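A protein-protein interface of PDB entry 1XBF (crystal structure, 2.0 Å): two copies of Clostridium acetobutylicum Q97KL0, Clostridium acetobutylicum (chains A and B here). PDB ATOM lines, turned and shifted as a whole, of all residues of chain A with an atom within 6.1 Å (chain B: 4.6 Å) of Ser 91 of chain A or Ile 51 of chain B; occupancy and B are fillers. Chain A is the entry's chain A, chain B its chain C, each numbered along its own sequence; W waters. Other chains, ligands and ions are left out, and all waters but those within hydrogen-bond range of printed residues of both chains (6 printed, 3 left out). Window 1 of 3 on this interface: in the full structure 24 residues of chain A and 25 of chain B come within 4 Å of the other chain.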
ATOM      1  N   PHE A  41      30.744  22.581   9.117  1.00  0.00           N
ATOM      2  CA  PHE A  41      29.545  23.396   9.079  1.00  0.00           C
ATOM      3  C   PHE A  41      28.712  23.170   7.829  1.00  0.00           C
ATOM      4  O   PHE A  41      29.240  23.068   6.717  1.00  0.00           O
ATOM      5  CB  PHE A  41      29.942  24.870   9.204  1.00  0.00           C
ATOM      6  CG  PHE A  41      28.786  25.808   9.304  1.00  0.00           C
ATOM      7  CD1 PHE A  41      28.076  26.193   8.168  1.00  0.00           C
ATOM      8  CD2 PHE A  41      28.388  26.304  10.544  1.00  0.00           C
ATOM      9  CE1 PHE A  41      26.986  27.056   8.264  1.00  0.00           C
ATOM     10  CE2 PHE A  41      27.301  27.165  10.654  1.00  0.00           C
ATOM     11  CZ  PHE A  41      26.596  27.544   9.514  1.00  0.00           C
ATOM     12  N   CYS A  42      27.400  23.087   8.022  1.00  0.00           N
ATOM     13  CA  CYS A  42      26.463  22.875   6.925  1.00  0.00           C
ATOM     14  C   CYS A  42      25.694  24.170   6.695  1.00  0.00           C
ATOM     15  O   CYS A  42      24.912  24.602   7.546  1.00  0.00           O
ATOM     16  CB  CYS A  42      25.502  21.733   7.271  1.00  0.00           C
ATOM     17  SG  CYS A  42      24.149  21.487   6.095  1.00  0.00           S
ATOM     18  N   HIS A  44      23.175  24.791   4.941  1.00  0.00           N
ATOM     19  CA  HIS A  44      21.802  24.586   4.488  1.00  0.00           C
ATOM     20  C   HIS A  44      20.822  24.476   5.651  1.00  0.00           C
ATOM     21  O   HIS A  44      21.175  23.994   6.730  1.00  0.00           O
ATOM     22  CB  HIS A  44      21.721  23.338   3.613  1.00  0.00           C
ATOM     23  CG  HIS A  44      22.721  23.327   2.498  1.00  0.00           C
ATOM     24  ND1 HIS A  44      24.027  22.925   2.675  1.00  0.00           N
ATOM     25  CD2 HIS A  44      22.624  23.730   1.209  1.00  0.00           C
ATOM     26  CE1 HIS A  44      24.692  23.081   1.544  1.00  0.00           C
ATOM     27  NE2 HIS A  44      23.864  23.569   0.638  1.00  0.00           N
ATOM     28  N   THR A  45      19.590  24.919   5.425  1.00  0.00           N
ATOM     29  CA  THR A  45      18.556  24.884   6.459  1.00  0.00           C
ATOM     30  C   THR A  45      17.672  23.646   6.384  1.00  0.00           C
ATOM     31  O   THR A  45      16.771  23.484   7.200  1.00  0.00           O
ATOM     32  CB  THR A  45      17.640  26.122   6.385  1.00  0.00           C
ATOM     33  OG1 THR A  45      17.052  26.207   5.081  1.00  0.00           O
ATOM     34  CG2 THR A  45      18.428  27.391   6.678  1.00  0.00           C
ATOM     35  N   ALA A  47      19.241  20.578   5.900  1.00  0.00           N
ATOM     36  CA  ALA A  47      20.265  19.556   6.053  1.00  0.00           C
ATOM     37  C   ALA A  47      21.073  19.929   7.289  1.00  0.00           C
ATOM     38  O   ALA A  47      20.926  21.022   7.829  1.00  0.00           O
ATOM     39  CB  ALA A  47      21.177  19.516   4.823  1.00  0.00           C
ATOM     40  N   ALA A  86      11.823  18.894   6.978  1.00  0.00           N
ATOM     41  CA  ALA A  86      13.265  18.867   6.772  1.00  0.00           C
ATOM     42  C   ALA A  86      13.938  19.955   7.604  1.00  0.00           C
ATOM     43  O   ALA A  86      15.047  19.761   8.103  1.00  0.00           O
ATOM     44  CB  ALA A  86      13.597  19.062   5.288  1.00  0.00           C
ATOM     45  N   HIS A  87      13.269  21.099   7.739  1.00  0.00           N
ATOM     46  CA  HIS A  87      13.800  22.213   8.528  1.00  0.00           C
ATOM     47  C   HIS A  87      13.878  21.810   9.992  1.00  0.00           C
ATOM     48  O   HIS A  87      14.815  22.168  10.693  1.00  0.00           O
ATOM     49  CB  HIS A  87      12.908  23.462   8.411  1.00  0.00           C
ATOM     50  CG  HIS A  87      13.095  24.231   7.139  1.00  0.00           C
ATOM     51  ND1 HIS A  87      12.170  24.223   6.117  1.00  0.00           N
ATOM     52  CD2 HIS A  87      14.112  25.019   6.721  1.00  0.00           C
ATOM     53  CE1 HIS A  87      12.609  24.971   5.120  1.00  0.00           C
ATOM     54  NE2 HIS A  87      13.785  25.465   5.460  1.00  0.00           N
ATOM     55  N   ILE A  88      12.886  21.061  10.450  1.00  0.00           N
ATOM     56  CA  ILE A  88      12.858  20.635  11.845  1.00  0.00           C
ATOM     57  C   ILE A  88      14.003  19.672  12.121  1.00  0.00           C
ATOM     58  O   ILE A  88      14.760  19.853  13.072  1.00  0.00           O
ATOM     59  CB  ILE A  88      11.534  19.938  12.190  1.00  0.00           C
ATOM     60  CG1 ILE A  88      10.380  20.933  12.053  1.00  0.00           C
ATOM     61  CG2 ILE A  88      11.601  19.361  13.620  1.00  0.00           C
ATOM     62  CD1 ILE A  88       8.983  20.296  12.103  1.00  0.00           C
ATOM     63  N   LYS A  89      14.127  18.661  11.268  1.00  0.00           N
ATOM     64  CA  LYS A  89      15.163  17.643  11.411  1.00  0.00           C
ATOM     65  C   LYS A  89      16.555  18.232  11.286  1.00  0.00           C
ATOM     66  O   LYS A  89      17.503  17.746  11.907  1.00  0.00           O
ATOM     67  CB  LYS A  89      14.970  16.546  10.367  1.00  0.00           C
ATOM     68  CG  LYS A  89      13.656  15.759  10.503  1.00  0.00           C
ATOM     69  CD  LYS A  89      13.517  14.821   9.308  1.00  0.00           C
ATOM     70  CE  LYS A  89      12.127  14.230   9.176  1.00  0.00           C
ATOM     71  NZ  LYS A  89      12.064  13.412   7.922  1.00  0.00           N
ATOM     72  N   ALA A  90      16.681  19.275  10.474  1.00  0.00           N
ATOM     73  CA  ALA A  90      17.964  19.943  10.292  1.00  0.00           C
ATOM     74  C   ALA A  90      18.395  20.522  11.644  1.00  0.00           C
ATOM     75  O   ALA A  90      19.523  20.319  12.083  1.00  0.00           O
ATOM     76  CB  ALA A  90      17.828  21.062   9.239  1.00  0.00           C
ATOM     77  N   SER A  91      17.490  21.236  12.305  1.00  0.00           N
ATOM     78  CA  SER A  91      17.794  21.814  13.609  1.00  0.00           C
ATOM     79  C   SER A  91      18.078  20.731  14.655  1.00  0.00           C
ATOM     80  O   SER A  91      18.885  20.947  15.550  1.00  0.00           O
ATOM     81  CB  SER A  91      16.644  22.701  14.094  1.00  0.00           C
ATOM     82  OG  SER A  91      16.777  24.035  13.624  1.00  0.00           O
ATOM     83  N   LEU A  92      17.419  19.577  14.542  1.00  0.00           N
ATOM     84  CA  LEU A  92      17.632  18.480  15.485  1.00  0.00           C
ATOM     85  C   LEU A  92      19.027  17.893  15.363  1.00  0.00           C
ATOM     86  O   LEU A  92      19.651  17.576  16.375  1.00  0.00           O
ATOM     87  CB  LEU A  92      16.604  17.357  15.279  1.00  0.00           C
ATOM     88  CG  LEU A  92      15.148  17.738  15.532  1.00  0.00           C
ATOM     89  CD1 LEU A  92      14.264  16.517  15.337  1.00  0.00           C
ATOM     90  CD2 LEU A  92      14.992  18.297  16.948  1.00  0.00           C
ATOM     91  N   MET A  93      19.516  17.719  14.133  1.00  0.00           N
ATOM     92  CA  MET A  93      20.852  17.165  13.944  1.00  0.00           C
ATOM     93  C   MET A  93      21.901  18.213  14.294  1.00  0.00           C
ATOM     94  O   MET A  93      22.910  17.896  14.922  1.00  0.00           O
ATOM     95  CB  MET A  93      21.063  16.679  12.510  1.00  0.00           C
ATOM     96  CG  MET A  93      20.168  15.515  12.113  1.00  0.00           C
ATOM     97  SD  MET A  93      20.383  13.863  13.120  1.00  0.00           S
ATOM     98  CE  MET A  93      18.986  14.165  14.457  1.00  0.00           C
ATOM     99  N   GLY A  94      21.643  19.461  13.909  1.00  0.00           N
ATOM    100  CA  GLY A  94      22.564  20.548  14.197  1.00  0.00           C
ATOM    101  C   GLY A  94      23.199  21.085  12.928  1.00  0.00           C
ATOM    102  O   GLY A  94      23.362  20.343  11.961  1.00  0.00           O
ATOM    103  N   SER A  95      23.569  22.364  12.933  1.00  0.00           N
ATOM    104  CA  SER A  95      24.174  22.998  11.758  1.00  0.00           C
ATOM    105  C   SER A  95      25.672  22.736  11.646  1.00  0.00           C
ATOM    106  O   SER A  95      26.283  22.991  10.608  1.00  0.00           O
ATOM    107  CB  SER A  95      23.900  24.507  11.784  1.00  0.00           C
ATOM    108  OG  SER A  95      24.273  25.067  13.033  1.00  0.00           O
ATOM    109  N   THR B  50      19.774  27.932  17.737  1.00  0.00           N
ATOM    110  CA  THR B  50      19.749  27.115  16.533  1.00  0.00           C
ATOM    111  C   THR B  50      19.920  28.011  15.311  1.00  0.00           C
ATOM    112  O   THR B  50      19.819  29.232  15.407  1.00  0.00           O
ATOM    113  CB  THR B  50      18.443  26.311  16.373  1.00  0.00           C
ATOM    114  OG1 THR B  50      18.613  25.354  15.315  1.00  0.00           O
ATOM    115  CG2 THR B  50      17.280  27.220  16.026  1.00  0.00           C
ATOM    116  N   ILE B  51      20.196  27.394  14.170  1.00  0.00           N
ATOM    117  CA  ILE B  51      20.375  28.118  12.917  1.00  0.00           C
ATOM    118  C   ILE B  51      19.389  27.521  11.913  1.00  0.00           C
ATOM    119  O   ILE B  51      19.400  26.312  11.678  1.00  0.00           O
ATOM    120  CB  ILE B  51      21.827  27.947  12.383  1.00  0.00           C
ATOM    121  CG1 ILE B  51      22.833  28.573  13.360  1.00  0.00           C
ATOM    122  CG2 ILE B  51      21.963  28.596  11.010  1.00  0.00           C
ATOM    123  CD1 ILE B  51      24.292  28.341  12.959  1.00  0.00           C
ATOM    124  N   ASN B  52      18.525  28.350  11.333  1.00  0.00           N
ATOM    125  CA  ASN B  52      17.562  27.840  10.362  1.00  0.00           C
ATOM    126  C   ASN B  52      17.053  28.949   9.426  1.00  0.00           C
ATOM    127  O   ASN B  52      17.566  30.067   9.441  1.00  0.00           O
ATOM    128  CB  ASN B  52      16.388  27.170  11.102  1.00  0.00           C
ATOM    129  CG  ASN B  52      15.819  25.978  10.345  1.00  0.00           C
ATOM    130  OD1 ASN B  52      15.226  26.134   9.279  1.00  0.00           O
ATOM    131  ND2 ASN B  52      15.998  24.774  10.898  1.00  0.00           N
ATOM    132  N   ILE B  63       8.355  24.922  13.297  1.00  0.00           N
ATOM    133  CA  ILE B  63       9.265  24.237  14.199  1.00  0.00           C
ATOM    134  C   ILE B  63       8.726  24.310  15.616  1.00  0.00           C
ATOM    135  O   ILE B  63       8.669  23.307  16.311  1.00  0.00           O
ATOM    136  CB  ILE B  63      10.680  24.847  14.174  1.00  0.00           C
ATOM    137  CG1 ILE B  63      11.268  24.717  12.766  1.00  0.00           C
ATOM    138  CG2 ILE B  63      11.569  24.132  15.215  1.00  0.00           C
ATOM    139  CD1 ILE B  63      12.568  25.479  12.553  1.00  0.00           C
ATOM    140  N   LEU B  92      17.255  19.850  22.621  1.00  0.00           N
ATOM    141  CA  LEU B  92      17.127  19.426  21.219  1.00  0.00           C
ATOM    142  C   LEU B  92      17.711  20.494  20.289  1.00  0.00           C
ATOM    143  O   LEU B  92      18.337  20.173  19.282  1.00  0.00           O
ATOM    144  CB  LEU B  92      15.650  19.161  20.867  1.00  0.00           C
ATOM    145  CG  LEU B  92      14.997  17.959  21.597  1.00  0.00           C
ATOM    146  CD1 LEU B  92      13.514  17.843  21.246  1.00  0.00           C
ATOM    147  CD2 LEU B  92      15.723  16.674  21.191  1.00  0.00           C
ATOM    148  N   MET B  93      17.508  21.757  20.634  1.00  0.00           N
ATOM    149  CA  MET B  93      18.030  22.859  19.831  1.00  0.00           C
ATOM    150  C   MET B  93      19.524  22.988  20.115  1.00  0.00           C
ATOM    151  O   MET B  93      20.325  23.184  19.198  1.00  0.00           O
ATOM    152  CB  MET B  93      17.320  24.169  20.196  1.00  0.00           C
ATOM    153  CG  MET B  93      15.837  24.227  19.840  1.00  0.00           C
ATOM    154  SD  MET B  93      15.479  23.970  17.919  1.00  0.00           S
ATOM    155  CE  MET B  93      15.242  22.050  17.915  1.00  0.00           C
ATOM    156  N   GLN B  97      25.806  27.302  19.331  1.00  0.00           N
ATOM    157  CA  GLN B  97      26.051  27.025  17.927  1.00  0.00           C
ATOM    158  C   GLN B  97      27.332  27.775  17.531  1.00  0.00           C
ATOM    159  O   GLN B  97      27.715  28.761  18.170  1.00  0.00           O
ATOM    160  CB  GLN B  97      24.854  27.453  17.071  1.00  0.00           C
ATOM    161  CG  GLN B  97      23.524  26.736  17.432  1.00  0.00           C
ATOM    162  CD  GLN B  97      23.586  25.208  17.328  1.00  0.00           C
ATOM    163  OE1 GLN B  97      22.672  24.510  17.791  1.00  0.00           O
ATOM    164  NE2 GLN B  97      24.646  24.684  16.713  1.00  0.00           N
ATOM    165  N   GLN B  98      27.997  27.283  16.491  1.00  0.00           N
ATOM    166  CA  GLN B  98      29.253  27.858  16.019  1.00  0.00           C
ATOM    167  C   GLN B  98      29.133  28.335  14.586  1.00  0.00           C
ATOM    168  O   GLN B  98      28.514  27.670  13.757  1.00  0.00           O
ATOM    169  CB  GLN B  98      30.355  26.801  16.102  1.00  0.00           C
ATOM    170  CG  GLN B  98      31.559  27.193  16.914  1.00  0.00           C
ATOM    171  CD  GLN B  98      32.528  26.039  17.094  1.00  0.00           C
ATOM    172  OE1 GLN B  98      33.538  26.162  17.785  1.00  0.00           O
ATOM    173  NE2 GLN B  98      32.220  24.905  16.471  1.00  0.00           N
ATOM    174  N   ILE B  99      29.731  29.488  14.290  1.00  0.00           N
ATOM    175  CA  ILE B  99      29.698  30.034  12.947  1.00  0.00           C
ATOM    176  C   ILE B  99      31.096  30.450  12.474  1.00  0.00           C
ATOM    177  O   ILE B  99      31.837  31.132  13.183  1.00  0.00           O
ATOM    178  CB  ILE B  99      28.754  31.249  12.841  1.00  0.00           C
ATOM    179  CG1 ILE B  99      27.358  30.916  13.400  1.00  0.00           C
ATOM    180  CG2 ILE B  99      28.602  31.635  11.384  1.00  0.00           C
ATOM    181  CD1 ILE B  99      27.195  31.142  14.899  1.00  0.00           C
ATOM    182  N   LEU B 108      27.677  32.239   6.685  1.00  0.00           N
ATOM    183  CA  LEU B 108      26.372  31.592   6.751  1.00  0.00           C
ATOM    184  C   LEU B 108      25.791  31.318   5.374  1.00  0.00           C
ATOM    185  O   LEU B 108      26.158  31.968   4.391  1.00  0.00           O
ATOM    186  CB  LEU B 108      25.390  32.477   7.513  1.00  0.00           C
ATOM    187  CG  LEU B 108      25.498  32.615   9.029  1.00  0.00           C
ATOM    188  CD1 LEU B 108      24.608  33.754   9.494  1.00  0.00           C
ATOM    189  CD2 LEU B 108      25.090  31.314   9.690  1.00  0.00           C
ATOM    190  N   GLN B 112      20.282  31.170   6.033  1.00  0.00           N
ATOM    191  CA  GLN B 112      20.544  30.867   7.439  1.00  0.00           C
ATOM    192  C   GLN B 112      20.573  32.055   8.393  1.00  0.00           C
ATOM    193  O   GLN B 112      21.335  33.005   8.210  1.00  0.00           O
ATOM    194  CB  GLN B 112      21.864  30.122   7.602  1.00  0.00           C
ATOM    195  CG  GLN B 112      21.868  28.699   7.113  1.00  0.00           C
ATOM    196  CD  GLN B 112      23.164  28.007   7.470  1.00  0.00           C
ATOM    197  OE1 GLN B 112      24.247  28.579   7.310  1.00  0.00           O
ATOM    198  NE2 GLN B 112      23.068  26.776   7.951  1.00  0.00           N
ATOM    199  N   GLY B 113      19.732  31.979   9.417  1.00  0.00           N
ATOM    200  CA  GLY B 113      19.701  33.009  10.429  1.00  0.00           C
ATOM    201  C   GLY B 113      20.031  32.312  11.739  1.00  0.00           C
ATOM    202  O   GLY B 113      19.767  31.110  11.883  1.00  0.00           O
ATOM    203  N   ILE B 114      20.633  33.036  12.675  1.00  0.00           N
ATOM    204  CA  ILE B 114      20.957  32.483  13.980  1.00  0.00           C
ATOM    205  C   ILE B 114      19.807  32.859  14.912  1.00  0.00           C
ATOM    206  O   ILE B 114      19.454  34.030  15.032  1.00  0.00           O
ATOM    207  CB  ILE B 114      22.263  33.068  14.527  1.00  0.00           C
ATOM    208  CG1 ILE B 114      23.395  32.836  13.522  1.00  0.00           C
ATOM    209  CG2 ILE B 114      22.600  32.424  15.858  1.00  0.00           C
ATOM    210  CD1 ILE B 114      24.712  33.433  13.934  1.00  0.00           C
HETATM  211  O   HOH W   1      20.408  23.724  12.591  1.00  0.00           O
HETATM  212  O   HOH W   2      20.821  25.563   9.056  1.00  0.00           O
HETATM  213  O   HOH W   3      18.075  17.557  18.615  1.00  0.00           O
HETATM  214  O   HOH W   4      22.196  24.329  14.533  1.00  0.00           O
HETATM  215  O   HOH W   5      24.992  21.900  15.775  1.00  0.00           O
HETATM  216  O   HOH W   6      27.007  25.530  14.282  1.00  0.00           O
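O of Ser 95 of chain A lies within hydrogen-bond range of N of Cys 42 of chain A (2.8 Å).
The side-chain hydroxyl (OG1) of Thr 45 of chain A is in hydrogen-bond range of a ring nitrogen (NE2) of His 87 of chain A.
The side-chain amide oxygen (OE1) of Gln 97 of chain B lies close to the backbone carbonyl oxygen (O) of Met 93 of chain B, at 3.0 Å.
O of Ala 47 of chain A sits close to SG of Cys 42 of chain A (3.7 Å).
O of Asn 52 of chain B lies within hydrogen-bond range of N of Gly 113 of chain B (2.9 Å).
The side-chain sulfur (SG) of Cys 42 of chain A lies close to the backbone NH (N) of His 44 of chain A (3.6 Å).
Hydrophobic or aromatic side chains of chain B within 4 Å of the printed part of chain A: Ile 51, Ile 63 and Met 93.
Among the printed residues, 16 pairs touch across the chains.
Among the printed residues, no Asp or Glu carboxylate lies within 4 Å of a Lys or Arg side-chain nitrogen of the other chain.
Printed residues of chain B within 4 Å of Thr 45 of chain A: Asn 52 (3.4 Å) and Gln 112 (3.7 Å).
Of the printed residues of chain B, Ser 91 of chain A touches Thr 50 (2.8 Å), Ile 51 (3.98 Å), Asn 52 (2.9 Å) and Leu 92 (3.9 Å).
Printed residues of chain A within 4 Å of Thr 50 of chain B: Ser 91.
Of the printed residues of chain A, Ile 51 of chain B touches Phe 41 (3.97 Å), Ser 91 (3.98 Å) and Ser 95 (3.3 Å).
Of the printed residues of chain A, Ile 63 of chain B touches Ile 88 (3.95 Å).
The nearest printed residue of chain B that does not touch Ser 91 of chain A is Met 93 of chain B (4.1 Å).
The nearest printed residue of chain B that does not touch Thr 45 of chain A is Ile 51 of chain B (5.2 Å).
OG of Ser 91 of chain A lies within hydrogen-bond range of OG1 of Thr 50 of chain B, at 2.8 Å.
O of His 87 of chain A is in hydrogen-bond range of ND2 of Asn 52 of chain B, 2.9 Å away.
The side-chain amide nitrogen (NE2) of Gln 112 of chain B is in hydrogen-bond range of the backbone carbonyl oxygen (O) of Cys 42 of chain A (2.9 Å).
The side-chain hydroxyl (OG) of Ser 91 of chain A is in hydrogen-bond range of the side-chain amide nitrogen (ND2) of Asn 52 of chain B, 2.9 Å away.
Water W4 lies within hydrogen-bond range of OG of Ser 95 of chain A and OE1 of Gln 97 of chain B.
Water W6 lies within hydrogen-bond range of O of Gln 98 of chain B (2.7 Å), OG of Ser 95 of chain A (3.0 Å) and NE2 of Gln 97 of chain B (3.5 Å).
Water W3 bridges the backbone carbonyl oxygen (O) of Leu 92 of chain B (2.7 Å) and the backbone carbonyl oxygen (O) of Leu 92 of chain A (2.7 Å).
Water W2 lies within hydrogen-bond range of NE2 of Gln 112 of chain B (2.8 Å), O of His 44 of chain A (2.8 Å) and O of Ile 51 of chain B (3.1 Å).
Water W1 lies within hydrogen-bond range of the backbone carbonyl oxygen of Ile 51 of chain B (2.9 Å) and the backbone NH of Ser 95 of chain A (3.5 Å).
Water W5 lies within hydrogen-bond range of the side-chain amide nitrogen (NE2) of Gln 97 of chain B and the backbone NH (N) of Ser 95 of chain A.
Among the printed residues, merely in contact across the chains: Phe 41 of chain A with Ile 51 of chain B, Phe 41 of chain A with Gln 98 of chain B, Phe 41 of chain A with Gln 112 of chain B, His 44 of chain A with Gln 112 of chain B, Thr 45 of chain A with Asn 52 of chain B, Thr 45 of chain A with Gln 112 of chain B, Ile 88 of chain A with Ile 63 of chain B, Ser 91 of chain A with Ile 51 of chain B, Ser 91 of chain A with Leu 92 of chain B, Leu 92 of chain A with Met 93 of chain B, Ser 95 of chain A with Ile 51 of chain B and Ser 95 of chain A with Gln 97 of chain B.
Leu 92 of chain A touches Met 93 of chain B, but with the chains exchanged Met 93 of chain A does not touch Leu 92 of chain B (5.8 Å).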
